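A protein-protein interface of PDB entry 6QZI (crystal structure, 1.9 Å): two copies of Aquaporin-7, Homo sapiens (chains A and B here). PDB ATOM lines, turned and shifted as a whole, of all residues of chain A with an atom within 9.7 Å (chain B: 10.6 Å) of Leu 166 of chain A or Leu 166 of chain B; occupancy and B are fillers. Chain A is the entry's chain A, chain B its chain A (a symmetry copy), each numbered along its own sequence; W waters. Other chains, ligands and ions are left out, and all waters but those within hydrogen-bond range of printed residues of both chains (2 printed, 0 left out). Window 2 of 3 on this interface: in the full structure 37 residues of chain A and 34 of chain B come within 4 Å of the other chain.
A ring nitrogen (ND1) of His 51 of chain A lies within hydrogen-bond range of the backbone carbonyl oxygen of Asn 163 of chain B (2.8 Å).
The backbone carbonyl oxygen (O) of Gly 168 of chain A lies within hydrogen-bond range of the backbone NH (N) of Leu 166 of chain B (3.0 Å).
O of Ile 157 of chain B is in hydrogen-bond range of N of Ala 165 of chain B, 2.9 Å away.
N of Gly 168 of chain A lies within hydrogen-bond range of OE2 of Glu 170 of chain A, at 2.7 Å.
The backbone carbonyl oxygen (O) of Leu 166 of chain B sits at hydrogen-bond distance from the side-chain hydroxyl (OG1) of Thr 169 of chain B, 2.8 Å away.
The side-chain hydroxyl (OG1) of Thr 169 of chain A is in hydrogen-bond range of the backbone carbonyl oxygen (O) of Leu 166 of chain A (2.8 Å).
Among the printed residues, pairs that only touch across the chains: His 51 of chain A with Asn 162 of chain B (3.7 Å), His 51 of chain A with Pro 164 of chain B (3.7 Å), His 51 of chain A with Ala 165 of chain B (3.3 Å), His 51 of chain A with Val 173 of chain B (3.6 Å), Leu 166 of chain A with Leu 166 of chain B (3.6 Å), Pro 167 of chain A with Leu 166 of chain B (3.4 Å), Gly 168 of chain A with Ala 165 of chain B (3.7 Å) and Leu 172 of chain A with Val 173 of chain B (3.99 Å).
Leu 166 of chain A touches one residue of chain B.
Printed residues of chain A within 4 Å of Leu 166 of chain B: Leu 166 (3.6 Å), Pro 167 (3.4 Å) and Gly 168 (3.0 Å).
No residue of chain B comes within 4 Å of Pro 164 of chain A.
Ala 165 of chain A touches none of the printed residues of chain B.
Of chain B, only Leu 166 (3.4 Å) comes within 4 Å of Pro 167 of chain A.
Gly 168 of chain A touches two residues of chain B.
No residue of chain B comes within 4 Å of Thr 169 of chain A.
Ala 165 of chain B touches just these residues of chain A: His 51 (3.3 Å) and Gly 168 (3.7 Å).
Pro 167 of chain B touches none of the printed residues of chain A.
Printed residues of chain A within 4 Å of Asn 162 of chain B: His 51.
Of the printed residues of chain A, Pro 164 of chain B touches His 51.
Of the printed residues of chain B, His 51 of chain A touches Asn 162 (3.7 Å), Asn 163 (2.8 Å), Pro 164 (3.7 Å), Ala 165 (3.3 Å) and Val 173 (3.6 Å).
Of the printed residues of chain A, Asn 163 of chain B touches His 51 (2.8 Å).
Of the printed residues of chain A, Val 173 of chain B touches His 51 (3.6 Å) and Leu 172 (3.99 Å).
The nearest residue of chain B that does not touch Leu 166 of chain A is Thr 169 of chain B (6.9 Å).
Of the 18 printed residues of chain A, 5 touch a printed residue of chain B.
Along chain A the printed residues that touch a printed residue of chain B span positions 51 to 172.
Of the 20 printed residues of chain B, 6 touch a printed residue of chain A.
Among the printed residues, no Asp or Glu carboxylate lies within 4 Å of a Lys or Arg side-chain nitrogen of the other chain.
Leu 166 of chain A touches its own counterpart, Leu 166 of chain B.
Pro 167 of chain A touches Leu 166 of chain B, but with the chains exchanged Leu 166 of chain A does not touch Pro 167 of chain B (7.9 Å).
Gly 168 of chain A touches Ala 165 of chain B, but with the chains exchanged Ala 165 of chain A does not touch Gly 168 of chain B (14.0 Å).
Gly 168 of chain A touches Leu 166 of chain B, but with the chains exchanged Leu 166 of chain A does not touch Gly 168 of chain B (9.4 Å).
18 positions are printed for both chains.
Of the 10 pairs that touch across the chains among the printed residues, 1 has its exchanged pair printed and touching as well.
Water W1 lies within hydrogen-bond range of O of Ala 156 of chain B (2.5 Å), O of His 51 of chain A (2.7 Å), N of Asn 163 of chain B (2.9 Å) and ND2 of Asn 162 of chain B (3.0 Å).
Water W2 bridges the backbone carbonyl oxygen of Gly 168 of chain A (2.7 Å) and the side-chain hydroxyl of Thr 169 of chain B (2.9 Å).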
ATOM      1  N   HIS A  51     -16.806 -11.196  -6.466  1.00  0.00           N
ATOM      2  CA  HIS A  51     -17.500 -10.878  -7.711  1.00  0.00           C
ATOM      3  C   HIS A  51     -19.014 -10.904  -7.526  1.00  0.00           C
ATOM      4  O   HIS A  51     -19.731 -10.136  -8.178  1.00  0.00           O
ATOM      5  CB  HIS A  51     -17.074 -11.845  -8.817  1.00  0.00           C
ATOM      6  CG  HIS A  51     -15.773 -11.481  -9.461  1.00  0.00           C
ATOM      7  ND1 HIS A  51     -15.609 -10.338 -10.212  1.00  0.00           N
ATOM      8  CD2 HIS A  51     -14.569 -12.105  -9.458  1.00  0.00           C
ATOM      9  CE1 HIS A  51     -14.363 -10.270 -10.644  1.00  0.00           C
ATOM     10  NE2 HIS A  51     -13.710 -11.330 -10.202  1.00  0.00           N
ATOM     11  N   ALA A 156      -5.409  -2.158   2.552  1.00  0.00           N
ATOM     12  CA  ALA A 156      -4.370  -1.720   1.626  1.00  0.00           C
ATOM     13  C   ALA A 156      -4.734  -2.048   0.182  1.00  0.00           C
ATOM     14  O   ALA A 156      -4.443  -1.269  -0.733  1.00  0.00           O
ATOM     15  CB  ALA A 156      -3.034  -2.363   2.002  1.00  0.00           C
ATOM     16  N   ILE A 157      -5.372  -3.199  -0.044  1.00  0.00           N
ATOM     17  CA  ILE A 157      -5.713  -3.605  -1.405  1.00  0.00           C
ATOM     18  C   ILE A 157      -6.822  -2.730  -1.975  1.00  0.00           C
ATOM     19  O   ILE A 157      -6.870  -2.488  -3.188  1.00  0.00           O
ATOM     20  CB  ILE A 157      -6.100  -5.097  -1.425  1.00  0.00           C
ATOM     21  CG1 ILE A 157      -4.888  -5.967  -1.085  1.00  0.00           C
ATOM     22  CG2 ILE A 157      -6.658  -5.505  -2.787  1.00  0.00           C
ATOM     23  CD1 ILE A 157      -5.251  -7.412  -0.768  1.00  0.00           C
ATOM     24  N   THR A 158      -7.714  -2.226  -1.128  1.00  0.00           N
ATOM     25  CA  THR A 158      -8.885  -1.495  -1.590  1.00  0.00           C
ATOM     26  C   THR A 158      -8.835   0.000  -1.296  1.00  0.00           C
ATOM     27  O   THR A 158      -9.798   0.708  -1.613  1.00  0.00           O
ATOM     28  CB  THR A 158     -10.154  -2.098  -0.972  1.00  0.00           C
ATOM     29  OG1 THR A 158     -10.073  -2.028   0.457  1.00  0.00           O
ATOM     30  CG2 THR A 158     -10.302  -3.559  -1.389  1.00  0.00           C
ATOM     31  N   ASP A 159      -7.743   0.505  -0.722  1.00  0.00           N
ATOM     32  CA  ASP A 159      -7.645   1.917  -0.342  1.00  0.00           C
ATOM     33  C   ASP A 159      -7.421   2.761  -1.591  1.00  0.00           C
ATOM     34  O   ASP A 159      -6.309   2.833  -2.117  1.00  0.00           O
ATOM     35  CB  ASP A 159      -6.525   2.123   0.671  1.00  0.00           C
ATOM     36  CG  ASP A 159      -6.489   3.536   1.234  1.00  0.00           C
ATOM     37  OD1 ASP A 159      -7.305   4.382   0.809  1.00  0.00           O
ATOM     38  OD2 ASP A 159      -5.640   3.799   2.110  1.00  0.00           O
ATOM     39  N   GLN A 160      -8.481   3.435  -2.046  1.00  0.00           N
ATOM     40  CA  GLN A 160      -8.414   4.280  -3.232  1.00  0.00           C
ATOM     41  C   GLN A 160      -7.525   5.501  -3.050  1.00  0.00           C
ATOM     42  O   GLN A 160      -7.190   6.153  -4.044  1.00  0.00           O
ATOM     43  CB  GLN A 160      -9.821   4.733  -3.627  1.00  0.00           C
ATOM     44  CG  GLN A 160     -10.778   3.589  -3.895  1.00  0.00           C
ATOM     45  CD  GLN A 160     -10.246   2.632  -4.937  1.00  0.00           C
ATOM     46  OE1 GLN A 160     -10.188   2.960  -6.122  1.00  0.00           O
ATOM     47  NE2 GLN A 160      -9.850   1.441  -4.503  1.00  0.00           N
ATOM     48  N   ASN A 163      -2.500   2.847  -2.475  1.00  0.00           N
ATOM     49  CA  ASN A 163      -2.000   2.080  -3.619  1.00  0.00           C
ATOM     50  C   ASN A 163      -2.845   0.821  -3.796  1.00  0.00           C
ATOM     51  O   ASN A 163      -2.393  -0.296  -3.541  1.00  0.00           O
ATOM     52  CB  ASN A 163      -0.525   1.722  -3.433  1.00  0.00           C
ATOM     53  CG  ASN A 163       0.078   1.098  -4.674  1.00  0.00           C
ATOM     54  OD1 ASN A 163      -0.329   1.405  -5.796  1.00  0.00           O
ATOM     55  ND2 ASN A 163       1.047   0.211  -4.482  1.00  0.00           N
ATOM     56  N   PRO A 164      -4.078   0.986  -4.259  1.00  0.00           N
ATOM     57  CA  PRO A 164      -4.995  -0.156  -4.331  1.00  0.00           C
ATOM     58  C   PRO A 164      -4.757  -0.986  -5.585  1.00  0.00           C
ATOM     59  O   PRO A 164      -4.091  -0.567  -6.534  1.00  0.00           O
ATOM     60  CB  PRO A 164      -6.367   0.522  -4.378  1.00  0.00           C
ATOM     61  CG  PRO A 164      -6.106   1.788  -5.122  1.00  0.00           C
ATOM     62  CD  PRO A 164      -4.685   2.210  -4.802  1.00  0.00           C
ATOM     63  N   ALA A 165      -5.320  -2.190  -5.568  1.00  0.00           N
ATOM     64  CA  ALA A 165      -5.402  -2.982  -6.785  1.00  0.00           C
ATOM     65  C   ALA A 165      -6.237  -2.239  -7.819  1.00  0.00           C
ATOM     66  O   ALA A 165      -7.188  -1.529  -7.484  1.00  0.00           O
ATOM     67  CB  ALA A 165      -6.016  -4.351  -6.493  1.00  0.00           C
ATOM     68  N   LEU A 166      -5.864  -2.391  -9.084  1.00  0.00           N
ATOM     69  CA  LEU A 166      -6.611  -1.739 -10.150  1.00  0.00           C
ATOM     70  C   LEU A 166      -8.077  -2.155 -10.065  1.00  0.00           C
ATOM     71  O   LEU A 166      -8.367  -3.348  -9.891  1.00  0.00           O
ATOM     72  CB  LEU A 166      -6.030  -2.105 -11.514  1.00  0.00           C
ATOM     73  CG  LEU A 166      -6.594  -1.372 -12.731  1.00  0.00           C
ATOM     74  CD1 LEU A 166      -6.237   0.109 -12.696  1.00  0.00           C
ATOM     75  CD2 LEU A 166      -6.071  -2.014 -13.997  1.00  0.00           C
ATOM     76  N   PRO A 167      -9.017  -1.211 -10.124  1.00  0.00           N
ATOM     77  CA  PRO A 167     -10.437  -1.572 -10.035  1.00  0.00           C
ATOM     78  C   PRO A 167     -10.819  -2.607 -11.081  1.00  0.00           C
ATOM     79  O   PRO A 167     -10.488  -2.478 -12.264  1.00  0.00           O
ATOM     80  CB  PRO A 167     -11.153  -0.238 -10.266  1.00  0.00           C
ATOM     81  CG  PRO A 167     -10.181   0.785  -9.787  1.00  0.00           C
ATOM     82  CD  PRO A 167      -8.813   0.247 -10.108  1.00  0.00           C
ATOM     83  N   GLY A 168     -11.518  -3.645 -10.634  1.00  0.00           N
ATOM     84  CA  GLY A 168     -11.832  -4.782 -11.470  1.00  0.00           C
ATOM     85  C   GLY A 168     -10.889  -5.950 -11.303  1.00  0.00           C
ATOM     86  O   GLY A 168     -11.104  -6.992 -11.934  1.00  0.00           O
ATOM     87  N   THR A 169      -9.843  -5.804 -10.484  1.00  0.00           N
ATOM     88  CA  THR A 169      -8.942  -6.898 -10.158  1.00  0.00           C
ATOM     89  C   THR A 169      -8.787  -7.121  -8.660  1.00  0.00           C
ATOM     90  O   THR A 169      -8.017  -8.002  -8.264  1.00  0.00           O
ATOM     91  CB  THR A 169      -7.548  -6.660 -10.762  1.00  0.00           C
ATOM     92  OG1 THR A 169      -6.858  -5.663  -9.999  1.00  0.00           O
ATOM     93  CG2 THR A 169      -7.648  -6.204 -12.216  1.00  0.00           C
ATOM     94  N   GLU A 170      -9.488  -6.349  -7.821  1.00  0.00           N
ATOM     95  CA  GLU A 170      -9.331  -6.486  -6.375  1.00  0.00           C
ATOM     96  C   GLU A 170      -9.738  -7.870  -5.892  1.00  0.00           C
ATOM     97  O   GLU A 170      -9.153  -8.388  -4.934  1.00  0.00           O
ATOM     98  CB  GLU A 170     -10.151  -5.417  -5.646  1.00  0.00           C
ATOM     99  CG  GLU A 170      -9.853  -3.986  -6.073  1.00  0.00           C
ATOM    100  CD  GLU A 170     -10.898  -3.435  -7.026  1.00  0.00           C
ATOM    101  OE1 GLU A 170     -11.315  -2.267  -6.854  1.00  0.00           O
ATOM    102  OE2 GLU A 170     -11.304  -4.173  -7.947  1.00  0.00           O
ATOM    103  N   ALA A 171     -10.742  -8.479  -6.529  1.00  0.00           N
ATOM    104  CA  ALA A 171     -11.180  -9.813  -6.121  1.00  0.00           C
ATOM    105  C   ALA A 171     -10.040 -10.819  -6.213  1.00  0.00           C
ATOM    106  O   ALA A 171      -9.895 -11.695  -5.350  1.00  0.00           O
ATOM    107  CB  ALA A 171     -12.355 -10.268  -6.984  1.00  0.00           C
ATOM    108  N   LEU A 172      -9.214 -10.702  -7.252  1.00  0.00           N
ATOM    109  CA  LEU A 172      -8.076 -11.603  -7.409  1.00  0.00           C
ATOM    110  C   LEU A 172      -7.051 -11.388  -6.306  1.00  0.00           C
ATOM    111  O   LEU A 172      -6.573 -12.346  -5.687  1.00  0.00           O
ATOM    112  CB  LEU A 172      -7.428 -11.394  -8.778  1.00  0.00           C
ATOM    113  CG  LEU A 172      -8.154 -11.942 -10.002  1.00  0.00           C
ATOM    114  CD1 LEU A 172      -7.384 -11.590 -11.266  1.00  0.00           C
ATOM    115  CD2 LEU A 172      -8.317 -13.442  -9.872  1.00  0.00           C
ATOM    116  N   VAL A 173      -6.696 -10.127  -6.048  1.00  0.00           N
ATOM    117  CA  VAL A 173      -5.661  -9.831  -5.063  1.00  0.00           C
ATOM    118  C   VAL A 173      -6.131 -10.200  -3.662  1.00  0.00           C
ATOM    119  O   VAL A 173      -5.362 -10.735  -2.859  1.00  0.00           O
ATOM    120  CB  VAL A 173      -5.245  -8.351  -5.156  1.00  0.00           C
ATOM    121  CG1 VAL A 173      -4.026  -8.082  -4.281  1.00  0.00           C
ATOM    122  CG2 VAL A 173      -4.958  -7.971  -6.602  1.00  0.00           C
ATOM    123  N   ILE A 174      -7.395  -9.905  -3.341  1.00  0.00           N
ATOM    124  CA  ILE A 174      -7.952 -10.320  -2.056  1.00  0.00           C
ATOM    125  C   ILE A 174      -7.895 -11.835  -1.919  1.00  0.00           C
ATOM    126  O   ILE A 174      -7.549 -12.367  -0.856  1.00  0.00           O
ATOM    127  CB  ILE A 174      -9.392  -9.794  -1.903  1.00  0.00           C
ATOM    128  CG1 ILE A 174      -9.396  -8.275  -1.719  1.00  0.00           C
ATOM    129  CG2 ILE A 174     -10.091 -10.473  -0.728  1.00  0.00           C
ATOM    130  CD1 ILE A 174     -10.754  -7.638  -1.981  1.00  0.00           C
ATOM    131  N   VAL B  50     -11.081 -18.970 -23.967  1.00  0.00           N
ATOM    132  CA  VAL B  50     -11.798 -17.700 -23.901  1.00  0.00           C
ATOM    133  C   VAL B  50     -11.112 -16.654 -24.773  1.00  0.00           C
ATOM    134  O   VAL B  50     -11.773 -15.851 -25.441  1.00  0.00           O
ATOM    135  CB  VAL B  50     -11.932 -17.232 -22.440  1.00  0.00           C
ATOM    136  CG1 VAL B  50     -12.511 -15.818 -22.380  1.00  0.00           C
ATOM    137  CG2 VAL B  50     -12.817 -18.192 -21.659  1.00  0.00           C
ATOM    138  N   HIS B  51      -9.777 -16.650 -24.799  1.00  0.00           N
ATOM    139  CA  HIS B  51      -9.086 -15.705 -25.671  1.00  0.00           C
ATOM    140  C   HIS B  51      -9.345 -16.015 -27.143  1.00  0.00           C
ATOM    141  O   HIS B  51      -9.396 -15.096 -27.969  1.00  0.00           O
ATOM    142  CB  HIS B  51      -7.586 -15.710 -25.374  1.00  0.00           C
ATOM    143  CG  HIS B  51      -7.208 -14.877 -24.189  1.00  0.00           C
ATOM    144  ND1 HIS B  51      -7.345 -13.507 -24.170  1.00  0.00           N
ATOM    145  CD2 HIS B  51      -6.708 -15.222 -22.977  1.00  0.00           C
ATOM    146  CE1 HIS B  51      -6.947 -13.041 -23.000  1.00  0.00           C
ATOM    147  NE2 HIS B  51      -6.555 -14.060 -22.257  1.00  0.00           N
ATOM    148  N   ALA B 156     -21.435 -14.023 -12.548  1.00  0.00           N
ATOM    149  CA  ALA B 156     -20.912 -12.986 -11.664  1.00  0.00           C
ATOM    150  C   ALA B 156     -19.628 -12.376 -12.217  1.00  0.00           C
ATOM    151  O   ALA B 156     -19.396 -11.170 -12.083  1.00  0.00           O
ATOM    152  CB  ALA B 156     -20.674 -13.564 -10.269  1.00  0.00           C
ATOM    153  N   ILE B 157     -18.780 -13.196 -12.843  1.00  0.00           N
ATOM    154  CA  ILE B 157     -17.508 -12.695 -13.358  1.00  0.00           C
ATOM    155  C   ILE B 157     -17.724 -11.791 -14.564  1.00  0.00           C
ATOM    156  O   ILE B 157     -16.952 -10.850 -14.790  1.00  0.00           O
ATOM    157  CB  ILE B 157     -16.578 -13.878 -13.695  1.00  0.00           C
ATOM    158  CG1 ILE B 157     -16.179 -14.623 -12.420  1.00  0.00           C
ATOM    159  CG2 ILE B 157     -15.323 -13.404 -14.426  1.00  0.00           C
ATOM    160  CD1 ILE B 157     -15.535 -15.977 -12.687  1.00  0.00           C
ATOM    161  N   THR B 158     -18.773 -12.035 -15.345  1.00  0.00           N
ATOM    162  CA  THR B 158     -18.986 -11.315 -16.592  1.00  0.00           C
ATOM    163  C   THR B 158     -20.158 -10.341 -16.549  1.00  0.00           C
ATOM    164  O   THR B 158     -20.450  -9.706 -17.570  1.00  0.00           O
ATOM    165  CB  THR B 158     -19.189 -12.313 -17.741  1.00  0.00           C
ATOM    166  OG1 THR B 158     -20.322 -13.145 -17.461  1.00  0.00           O
ATOM    167  CG2 THR B 158     -17.953 -13.195 -17.898  1.00  0.00           C
ATOM    168  N   ASP B 159     -20.823 -10.186 -15.405  1.00  0.00           N
ATOM    169  CA  ASP B 159     -22.003  -9.324 -15.301  1.00  0.00           C
ATOM    170  C   ASP B 159     -21.562  -7.865 -15.282  1.00  0.00           C
ATOM    171  O   ASP B 159     -21.107  -7.352 -14.258  1.00  0.00           O
ATOM    172  CB  ASP B 159     -22.812  -9.670 -14.056  1.00  0.00           C
ATOM    173  CG  ASP B 159     -24.139  -8.929 -13.988  1.00  0.00           C
ATOM    174  OD1 ASP B 159     -24.423  -8.104 -14.882  1.00  0.00           O
ATOM    175  OD2 ASP B 159     -24.903  -9.178 -13.033  1.00  0.00           O
ATOM    176  N   GLN B 160     -21.735  -7.182 -16.417  1.00  0.00           N
ATOM    177  CA  GLN B 160     -21.357  -5.779 -16.546  1.00  0.00           C
ATOM    178  C   GLN B 160     -22.195  -4.850 -15.680  1.00  0.00           C
ATOM    179  O   GLN B 160     -21.817  -3.686 -15.510  1.00  0.00           O
ATOM    180  CB  GLN B 160     -21.466  -5.344 -18.008  1.00  0.00           C
ATOM    181  CG  GLN B 160     -20.617  -6.168 -18.955  1.00  0.00           C
ATOM    182  CD  GLN B 160     -19.163  -6.193 -18.544  1.00  0.00           C
ATOM    183  OE1 GLN B 160     -18.457  -5.191 -18.664  1.00  0.00           O
ATOM    184  NE2 GLN B 160     -18.704  -7.338 -18.052  1.00  0.00           N
ATOM    185  N   ASN B 162     -23.044  -5.668 -12.458  1.00  0.00           N
ATOM    186  CA  ASN B 162     -22.791  -5.971 -11.054  1.00  0.00           C
ATOM    187  C   ASN B 162     -21.341  -5.654 -10.700  1.00  0.00           C
ATOM    188  O   ASN B 162     -20.977  -4.483 -10.564  1.00  0.00           O
ATOM    189  CB  ASN B 162     -23.130  -7.433 -10.747  1.00  0.00           C
ATOM    190  CG  ASN B 162     -23.115  -7.733  -9.258  1.00  0.00           C
ATOM    191  OD1 ASN B 162     -23.042  -6.822  -8.433  1.00  0.00           O
ATOM    192  ND2 ASN B 162     -23.174  -9.015  -8.910  1.00  0.00           N
ATOM    193  N   ASN B 163     -20.505  -6.682 -10.540  1.00  0.00           N
ATOM    194  CA  ASN B 163     -19.097  -6.500 -10.181  1.00  0.00           C
ATOM    195  C   ASN B 163     -18.235  -7.456 -11.001  1.00  0.00           C
ATOM    196  O   ASN B 163     -17.680  -8.426 -10.482  1.00  0.00           O
ATOM    197  CB  ASN B 163     -18.882  -6.724  -8.683  1.00  0.00           C
ATOM    198  CG  ASN B 163     -17.480  -6.358  -8.241  1.00  0.00           C
ATOM    199  OD1 ASN B 163     -16.850  -5.466  -8.812  1.00  0.00           O
ATOM    200  ND2 ASN B 163     -16.978  -7.052  -7.227  1.00  0.00           N
ATOM    201  N   PRO B 164     -18.093  -7.180 -12.291  1.00  0.00           N
ATOM    202  CA  PRO B 164     -17.392  -8.121 -13.172  1.00  0.00           C
ATOM    203  C   PRO B 164     -15.883  -7.949 -13.085  1.00  0.00           C
ATOM    204  O   PRO B 164     -15.363  -6.956 -12.574  1.00  0.00           O
ATOM    205  CB  PRO B 164     -17.909  -7.726 -14.558  1.00  0.00           C
ATOM    206  CG  PRO B 164     -18.120  -6.254 -14.446  1.00  0.00           C
ATOM    207  CD  PRO B 164     -18.509  -5.966 -13.008  1.00  0.00           C
ATOM    208  N   ALA B 165     -15.180  -8.953 -13.601  1.00  0.00           N
ATOM    209  CA  ALA B 165     -13.751  -8.811 -13.828  1.00  0.00           C
ATOM    210  C   ALA B 165     -13.503  -7.686 -14.824  1.00  0.00           C
ATOM    211  O   ALA B 165     -14.295  -7.457 -15.741  1.00  0.00           O
ATOM    212  CB  ALA B 165     -13.158 -10.120 -14.350  1.00  0.00           C
ATOM    213  N   LEU B 166     -12.404  -6.968 -14.627  1.00  0.00           N
ATOM    214  CA  LEU B 166     -12.066  -5.884 -15.538  1.00  0.00           C
ATOM    215  C   LEU B 166     -11.996  -6.425 -16.963  1.00  0.00           C
ATOM    216  O   LEU B 166     -11.397  -7.488 -17.186  1.00  0.00           O
ATOM    217  CB  LEU B 166     -10.737  -5.246 -15.143  1.00  0.00           C
ATOM    218  CG  LEU B 166     -10.319  -3.982 -15.896  1.00  0.00           C
ATOM    219  CD1 LEU B 166     -11.256  -2.821 -15.586  1.00  0.00           C
ATOM    220  CD2 LEU B 166      -8.894  -3.625 -15.536  1.00  0.00           C
ATOM    221  N   PRO B 167     -12.633  -5.768 -17.932  1.00  0.00           N
ATOM    222  CA  PRO B 167     -12.597  -6.265 -19.313  1.00  0.00           C
ATOM    223  C   PRO B 167     -11.171  -6.451 -19.804  1.00  0.00           C
ATOM    224  O   PRO B 167     -10.316  -5.573 -19.648  1.00  0.00           O
ATOM    225  CB  PRO B 167     -13.332  -5.173 -20.098  1.00  0.00           C
ATOM    226  CG  PRO B 167     -14.264  -4.573 -19.102  1.00  0.00           C
ATOM    227  CD  PRO B 167     -13.555  -4.630 -17.776  1.00  0.00           C
ATOM    228  N   GLY B 168     -10.916  -7.612 -20.399  1.00  0.00           N
ATOM    229  CA  GLY B 168      -9.579  -8.002 -20.790  1.00  0.00           C
ATOM    230  C   GLY B 168      -8.882  -8.899 -19.796  1.00  0.00           C
ATOM    231  O   GLY B 168      -7.755  -9.332 -20.063  1.00  0.00           O
ATOM    232  N   THR B 169      -9.510  -9.179 -18.650  1.00  0.00           N
ATOM    233  CA  THR B 169      -8.986 -10.125 -17.677  1.00  0.00           C
ATOM    234  C   THR B 169      -9.980 -11.216 -17.306  1.00  0.00           C
ATOM    235  O   THR B 169      -9.655 -12.056 -16.460  1.00  0.00           O
ATOM    236  CB  THR B 169      -8.551  -9.403 -16.390  1.00  0.00           C
ATOM    237  OG1 THR B 169      -9.710  -9.033 -15.633  1.00  0.00           O
ATOM    238  CG2 THR B 169      -7.735  -8.152 -16.709  1.00  0.00           C
ATOM    239  N   GLU B 170     -11.175 -11.227 -17.907  1.00  0.00           N
ATOM    240  CA  GLU B 170     -12.183 -12.219 -17.543  1.00  0.00           C
ATOM    241  C   GLU B 170     -11.710 -13.636 -17.833  1.00  0.00           C
ATOM    242  O   GLU B 170     -12.063 -14.568 -17.102  1.00  0.00           O
ATOM    243  CB  GLU B 170     -13.494 -11.946 -18.287  1.00  0.00           C
ATOM    244  CG  GLU B 170     -14.050 -10.540 -18.099  1.00  0.00           C
ATOM    245  CD  GLU B 170     -13.761  -9.638 -19.285  1.00  0.00           C
ATOM    246  OE1 GLU B 170     -14.672  -8.893 -19.712  1.00  0.00           O
ATOM    247  OE2 GLU B 170     -12.622  -9.678 -19.793  1.00  0.00           O
ATOM    248  N   ALA B 171     -10.922 -13.822 -18.896  1.00  0.00           N
ATOM    249  CA  ALA B 171     -10.426 -15.157 -19.229  1.00  0.00           C
ATOM    250  C   ALA B 171      -9.616 -15.744 -18.080  1.00  0.00           C
ATOM    251  O   ALA B 171      -9.708 -16.944 -17.787  1.00  0.00           O
ATOM    252  CB  ALA B 171      -9.578 -15.101 -20.498  1.00  0.00           C
ATOM    253  N   LEU B 172      -8.820 -14.909 -17.414  1.00  0.00           N
ATOM    254  CA  LEU B 172      -8.027 -15.375 -16.280  1.00  0.00           C
ATOM    255  C   LEU B 172      -8.919 -15.783 -15.118  1.00  0.00           C
ATOM    256  O   LEU B 172      -8.743 -16.854 -14.527  1.00  0.00           O
ATOM    257  CB  LEU B 172      -7.053 -14.283 -15.838  1.00  0.00           C
ATOM    258  CG  LEU B 172      -5.829 -14.022 -16.710  1.00  0.00           C
ATOM    259  CD1 LEU B 172      -5.016 -12.871 -16.138  1.00  0.00           C
ATOM    260  CD2 LEU B 172      -4.990 -15.279 -16.805  1.00  0.00           C
ATOM    261  N   VAL B 173      -9.888 -14.931 -14.771  1.00  0.00           N
ATOM    262  CA  VAL B 173     -10.740 -15.201 -13.618  1.00  0.00           C
ATOM    263  C   VAL B 173     -11.621 -16.417 -13.874  1.00  0.00           C
ATOM    264  O   VAL B 173     -11.829 -17.245 -12.982  1.00  0.00           O
ATOM    265  CB  VAL B 173     -11.573 -13.954 -13.268  1.00  0.00           C
ATOM    266  CG1 VAL B 173     -12.307 -14.155 -11.947  1.00  0.00           C
ATOM    267  CG2 VAL B 173     -10.680 -12.722 -13.200  1.00  0.00           C
ATOM    268  N   ILE B 174     -12.166 -16.535 -15.089  1.00  0.00           N
ATOM    269  CA  ILE B 174     -12.937 -17.724 -15.446  1.00  0.00           C
ATOM    270  C   ILE B 174     -12.074 -18.972 -15.321  1.00  0.00           C
ATOM    271  O   ILE B 174     -12.520 -20.007 -14.812  1.00  0.00           O
ATOM    272  CB  ILE B 174     -13.515 -17.578 -16.867  1.00  0.00           C
ATOM    273  CG1 ILE B 174     -14.622 -16.523 -16.894  1.00  0.00           C
ATOM    274  CG2 ILE B 174     -14.046 -18.918 -17.370  1.00  0.00           C
ATOM    275  CD1 ILE B 174     -14.946 -16.023 -18.296  1.00  0.00           C
HETATM  276  O   HOH W   1     -20.745  -9.614 -10.594  1.00  0.00           O
HETATM  277  O   HOH W   2      -9.977  -9.263 -12.796  1.00  0.00           O
